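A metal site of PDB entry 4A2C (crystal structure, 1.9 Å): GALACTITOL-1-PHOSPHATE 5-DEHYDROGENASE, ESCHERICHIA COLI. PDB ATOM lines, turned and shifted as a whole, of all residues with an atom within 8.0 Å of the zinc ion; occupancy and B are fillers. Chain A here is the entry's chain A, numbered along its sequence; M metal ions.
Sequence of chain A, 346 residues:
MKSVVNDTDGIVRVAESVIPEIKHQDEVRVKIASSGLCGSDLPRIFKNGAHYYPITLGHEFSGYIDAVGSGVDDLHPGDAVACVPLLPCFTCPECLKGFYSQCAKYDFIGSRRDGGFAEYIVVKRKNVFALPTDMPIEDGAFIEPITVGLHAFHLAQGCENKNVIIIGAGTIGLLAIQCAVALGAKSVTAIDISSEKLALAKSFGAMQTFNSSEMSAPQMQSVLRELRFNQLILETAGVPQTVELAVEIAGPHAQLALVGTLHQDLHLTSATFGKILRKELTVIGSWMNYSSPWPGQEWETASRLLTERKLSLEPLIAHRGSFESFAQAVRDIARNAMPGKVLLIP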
ATOM      1  N   LEU A  87      17.383  26.236  10.347  1.00  0.00           N
ATOM      2  CA  LEU A  87      16.065  25.778  10.779  1.00  0.00           C
ATOM      3  C   LEU A  87      15.108  25.602   9.593  1.00  0.00           C
ATOM      4  O   LEU A  87      14.421  26.540   9.194  1.00  0.00           O
ATOM      5  CB  LEU A  87      15.431  26.712  11.827  1.00  0.00           C
ATOM      6  CG  LEU A  87      14.161  26.199  12.532  1.00  0.00           C
ATOM      7  CD1 LEU A  87      14.473  25.182  13.630  1.00  0.00           C
ATOM      8  CD2 LEU A  87      13.362  27.365  13.115  1.00  0.00           C
ATOM      9  N   PRO A  88      15.046  24.375   9.051  1.00  0.00           N
ATOM     10  CA  PRO A  88      14.091  24.122   7.965  1.00  0.00           C
ATOM     11  C   PRO A  88      12.681  24.139   8.540  1.00  0.00           C
ATOM     12  O   PRO A  88      12.575  24.193   9.774  1.00  0.00           O
ATOM     13  CB  PRO A  88      14.452  22.711   7.503  1.00  0.00           C
ATOM     14  CG  PRO A  88      15.009  22.056   8.724  1.00  0.00           C
ATOM     15  CD  PRO A  88      15.662  23.132   9.547  1.00  0.00           C
ATOM     16  N   CYS A  89      11.642  24.115   7.702  1.00  0.00           N
ATOM     17  CA  CYS A  89      10.256  24.153   8.173  1.00  0.00           C
ATOM     18  C   CYS A  89       9.793  22.812   8.714  1.00  0.00           C
ATOM     19  O   CYS A  89       8.915  22.759   9.588  1.00  0.00           O
ATOM     20  CB  CYS A  89       9.313  24.610   7.061  1.00  0.00           C
ATOM     21  SG  CYS A  89       8.968  23.290   5.829  1.00  0.00           S
ATOM     22  N   PHE A  90      10.410  21.742   8.188  1.00  0.00           N
ATOM     23  CA  PHE A  90      10.157  20.351   8.601  1.00  0.00           C
ATOM     24  C   PHE A  90       8.919  19.672   8.056  1.00  0.00           C
ATOM     25  O   PHE A  90       8.705  18.483   8.327  1.00  0.00           O
ATOM     26  CB  PHE A  90      10.161  20.223  10.123  1.00  0.00           C
ATOM     27  CG  PHE A  90      11.510  20.402  10.731  1.00  0.00           C
ATOM     28  CD1 PHE A  90      12.510  19.450  10.533  1.00  0.00           C
ATOM     29  CD2 PHE A  90      11.802  21.519  11.478  1.00  0.00           C
ATOM     30  CE1 PHE A  90      13.768  19.622  11.089  1.00  0.00           C
ATOM     31  CE2 PHE A  90      13.051  21.701  12.036  1.00  0.00           C
ATOM     32  CZ  PHE A  90      14.037  20.753  11.850  1.00  0.00           C
ATOM     33  N   THR A  91       8.099  20.387   7.291  1.00  0.00           N
ATOM     34  CA  THR A  91       6.802  19.843   6.902  1.00  0.00           C
ATOM     35  C   THR A  91       6.534  19.841   5.392  1.00  0.00           C
ATOM     36  O   THR A  91       5.539  19.293   4.941  1.00  0.00           O
ATOM     37  CB  THR A  91       5.669  20.605   7.602  1.00  0.00           C
ATOM     38  OG1 THR A  91       5.649  21.949   7.128  1.00  0.00           O
ATOM     39  CG2 THR A  91       5.874  20.596   9.105  1.00  0.00           C
ATOM     40  N   CYS A  92       7.417  20.460   4.620  1.00  0.00           N
ATOM     41  CA  CYS A  92       7.252  20.559   3.167  1.00  0.00           C
ATOM     42  C   CYS A  92       7.764  19.273   2.506  1.00  0.00           C
ATOM     43  O   CYS A  92       8.397  18.453   3.178  1.00  0.00           O
ATOM     44  CB  CYS A  92       8.021  21.778   2.638  1.00  0.00           C
ATOM     45  SG  CYS A  92       9.839  21.593   2.667  1.00  0.00           S
ATOM     46  N   PRO A  93       7.494  19.081   1.197  1.00  0.00           N
ATOM     47  CA  PRO A  93       7.927  17.796   0.658  1.00  0.00           C
ATOM     48  C   PRO A  93       9.447  17.577   0.788  1.00  0.00           C
ATOM     49  O   PRO A  93       9.857  16.475   1.159  1.00  0.00           O
ATOM     50  CB  PRO A  93       7.464  17.831  -0.815  1.00  0.00           C
ATOM     51  CG  PRO A  93       6.308  18.830  -0.812  1.00  0.00           C
ATOM     52  CD  PRO A  93       6.740  19.874   0.207  1.00  0.00           C
ATOM     53  N   GLU A  94      10.256  18.589   0.490  1.00  0.00           N
ATOM     54  CA  GLU A  94      11.698  18.461   0.676  1.00  0.00           C
ATOM     55  C   GLU A  94      12.086  17.983   2.089  1.00  0.00           C
ATOM     56  O   GLU A  94      12.849  17.019   2.222  1.00  0.00           O
ATOM     57  CB  GLU A  94      12.448  19.750   0.314  1.00  0.00           C
ATOM     58  CG  GLU A  94      12.529  20.020  -1.144  1.00  0.00           C
ATOM     59  CD  GLU A  94      11.255  20.592  -1.726  1.00  0.00           C
ATOM     60  OE1 GLU A  94      10.209  20.581  -1.041  1.00  0.00           O
ATOM     61  OE2 GLU A  94      11.303  21.063  -2.872  1.00  0.00           O
ATOM     62  N   CYS A  95      11.559  18.625   3.135  1.00  0.00           N
ATOM     63  CA  CYS A  95      11.850  18.203   4.509  1.00  0.00           C
ATOM     64  C   CYS A  95      11.369  16.797   4.835  1.00  0.00           C
ATOM     65  O   CYS A  95      12.066  16.044   5.501  1.00  0.00           O
ATOM     66  CB  CYS A  95      11.271  19.213   5.516  1.00  0.00           C
ATOM     67  SG  CYS A  95      12.106  20.839   5.488  1.00  0.00           S
ATOM     68  N   LEU A  96      10.177  16.427   4.351  1.00  0.00           N
ATOM     69  CA  LEU A  96       9.644  15.112   4.679  1.00  0.00           C
ATOM     70  C   LEU A  96      10.560  14.025   4.132  1.00  0.00           C
ATOM     71  O   LEU A  96      10.677  12.945   4.720  1.00  0.00           O
ATOM     72  CB  LEU A  96       8.221  14.923   4.137  1.00  0.00           C
ATOM     73  CG  LEU A  96       7.093  15.729   4.806  1.00  0.00           C
ATOM     74  CD1 LEU A  96       5.793  15.481   4.070  1.00  0.00           C
ATOM     75  CD2 LEU A  96       6.948  15.384   6.302  1.00  0.00           C
ATOM     76  N   PHE A  99      15.446  16.297   2.739  1.00  0.00           N
ATOM     77  CA  PHE A  99      16.181  17.289   1.969  1.00  0.00           C
ATOM     78  C   PHE A  99      16.099  18.670   2.646  1.00  0.00           C
ATOM     79  O   PHE A  99      15.721  19.660   2.010  1.00  0.00           O
ATOM     80  CB  PHE A  99      15.630  17.369   0.530  1.00  0.00           C
ATOM     81  CG  PHE A  99      15.727  16.066  -0.266  1.00  0.00           C
ATOM     82  CD1 PHE A  99      16.674  15.085   0.054  1.00  0.00           C
ATOM     83  CD2 PHE A  99      14.894  15.855  -1.352  1.00  0.00           C
ATOM     84  CE1 PHE A  99      16.774  13.915  -0.690  1.00  0.00           C
ATOM     85  CE2 PHE A  99      14.988  14.674  -2.118  1.00  0.00           C
ATOM     86  CZ  PHE A  99      15.922  13.706  -1.782  1.00  0.00           C
ATOM     87  N   TYR A 100      16.450  18.734   3.939  1.00  0.00           N
ATOM     88  CA  TYR A 100      16.268  19.968   4.706  1.00  0.00           C
ATOM     89  C   TYR A 100      17.008  21.161   4.086  1.00  0.00           C
ATOM     90  O   TYR A 100      16.560  22.304   4.182  1.00  0.00           O
ATOM     91  CB  TYR A 100      16.715  19.795   6.169  1.00  0.00           C
ATOM     92  CG  TYR A 100      16.234  18.533   6.844  1.00  0.00           C
ATOM     93  CD1 TYR A 100      14.907  18.376   7.234  1.00  0.00           C
ATOM     94  CD2 TYR A 100      17.121  17.491   7.125  1.00  0.00           C
ATOM     95  CE1 TYR A 100      14.470  17.200   7.870  1.00  0.00           C
ATOM     96  CE2 TYR A 100      16.699  16.333   7.754  1.00  0.00           C
ATOM     97  CZ  TYR A 100      15.382  16.192   8.120  1.00  0.00           C
ATOM     98  OH  TYR A 100      14.983  15.028   8.742  1.00  0.00           O
ATOM     99  N   SER A 101      18.133  20.884   3.428  1.00  0.00           N
ATOM    100  CA  SER A 101      18.973  21.929   2.861  1.00  0.00           C
ATOM    101  C   SER A 101      18.451  22.407   1.510  1.00  0.00           C
ATOM    102  O   SER A 101      19.071  23.272   0.889  1.00  0.00           O
ATOM    103  CB  SER A 101      20.416  21.453   2.739  1.00  0.00           C
ATOM    104  OG  SER A 101      20.899  21.040   4.004  1.00  0.00           O
ATOM    105  N   GLN A 102      17.337  21.822   1.052  1.00  0.00           N
ATOM    106  CA  GLN A 102      16.615  22.322  -0.110  1.00  0.00           C
ATOM    107  C   GLN A 102      15.256  22.853   0.322  1.00  0.00           C
ATOM    108  O   GLN A 102      14.361  23.036  -0.511  1.00  0.00           O
ATOM    109  CB  GLN A 102      16.423  21.238  -1.176  1.00  0.00           C
ATOM    110  CG  GLN A 102      17.686  20.893  -1.976  1.00  0.00           C
ATOM    111  CD  GLN A 102      18.636  20.018  -1.192  1.00  0.00           C
ATOM    112  OE1 GLN A 102      18.216  19.053  -0.548  1.00  0.00           O
ATOM    113  NE2 GLN A 102      19.932  20.364  -1.215  1.00  0.00           N
ATOM    114  N   CYS A 103      15.094  23.081   1.613  1.00  0.00           N
ATOM    115  CA  CYS A 103      13.857  23.709   2.070  1.00  0.00           C
ATOM    116  C   CYS A 103      13.897  25.179   1.665  1.00  0.00           C
ATOM    117  O   CYS A 103      14.917  25.847   1.878  1.00  0.00           O
ATOM    118  CB  CYS A 103      13.701  23.552   3.587  1.00  0.00           C
ATOM    119  SG  CYS A 103      12.215  24.336   4.316  1.00  0.00           S
ATOM    120  N   ALA A 104      12.798  25.676   1.102  1.00  0.00           N
ATOM    121  CA  ALA A 104      12.744  27.079   0.628  1.00  0.00           C
ATOM    122  C   ALA A 104      12.304  28.081   1.696  1.00  0.00           C
ATOM    123  O   ALA A 104      12.499  29.302   1.539  1.00  0.00           O
ATOM    124  CB  ALA A 104      11.846  27.186  -0.587  1.00  0.00           C
ATOM    125  N   LYS A 105      11.707  27.584   2.763  1.00  0.00           N
ATOM    126  CA  LYS A 105      11.262  28.469   3.826  1.00  0.00           C
ATOM    127  C   LYS A 105      12.101  28.249   5.081  1.00  0.00           C
ATOM    128  O   LYS A 105      11.674  27.557   6.020  1.00  0.00           O
ATOM    129  CB  LYS A 105       9.778  28.260   4.119  1.00  0.00           C
ATOM    130  CG  LYS A 105       8.871  28.642   2.959  1.00  0.00           C
ATOM    131  CD  LYS A 105       7.423  28.789   3.404  1.00  0.00           C
ATOM    132  CE  LYS A 105       6.559  29.514   2.363  1.00  0.00           C
ATOM    133  NZ  LYS A 105       6.789  30.989   2.352  1.00  0.00           N
ATOM    134  N   TYR A 106      13.298  28.828   5.114  1.00  0.00           N
ATOM    135  CA  TYR A 106      14.269  28.501   6.158  1.00  0.00           C
ATOM    136  C   TYR A 106      14.768  29.704   6.956  1.00  0.00           C
ATOM    137  O   TYR A 106      14.751  30.835   6.479  1.00  0.00           O
ATOM    138  CB  TYR A 106      15.469  27.759   5.561  1.00  0.00           C
ATOM    139  CG  TYR A 106      16.315  28.589   4.625  1.00  0.00           C
ATOM    140  CD1 TYR A 106      17.343  29.387   5.117  1.00  0.00           C
ATOM    141  CD2 TYR A 106      16.089  28.575   3.250  1.00  0.00           C
ATOM    142  CE1 TYR A 106      18.126  30.155   4.254  1.00  0.00           C
ATOM    143  CE2 TYR A 106      16.870  29.329   2.389  1.00  0.00           C
ATOM    144  CZ  TYR A 106      17.883  30.117   2.894  1.00  0.00           C
ATOM    145  OH  TYR A 106      18.642  30.869   2.036  1.00  0.00           O
HETATM  146 ZN    ZN M   1      10.774  22.498   4.586  1.00  0.00          ZN
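The side-chain sulfur of Cys 95 sits close to the backbone NH of Phe 90, at 3.3 Å.
SG of Cys 92 sits close to N of Glu 94, 3.7 Å away.
The backbone NH (N) of Thr 91 lies close to the side-chain sulfur (SG) of Cys 89, 3.4 Å away.
The side-chain sulfur of Cys 103 lies close to the backbone NH of Lys 105 (3.6 Å).
Merely in contact with the zinc ion: Phe 90 (3.7 Å).
Of the 18 residues printed, 5 come within 4 Å of the zinc ion.
The zinc ion is bound by SG of Cys 95 (2.3 Å), SG of Cys 92 (2.3 Å), SG of Cys 89 (2.3 Å) and SG of Cys 103 (2.4 Å).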
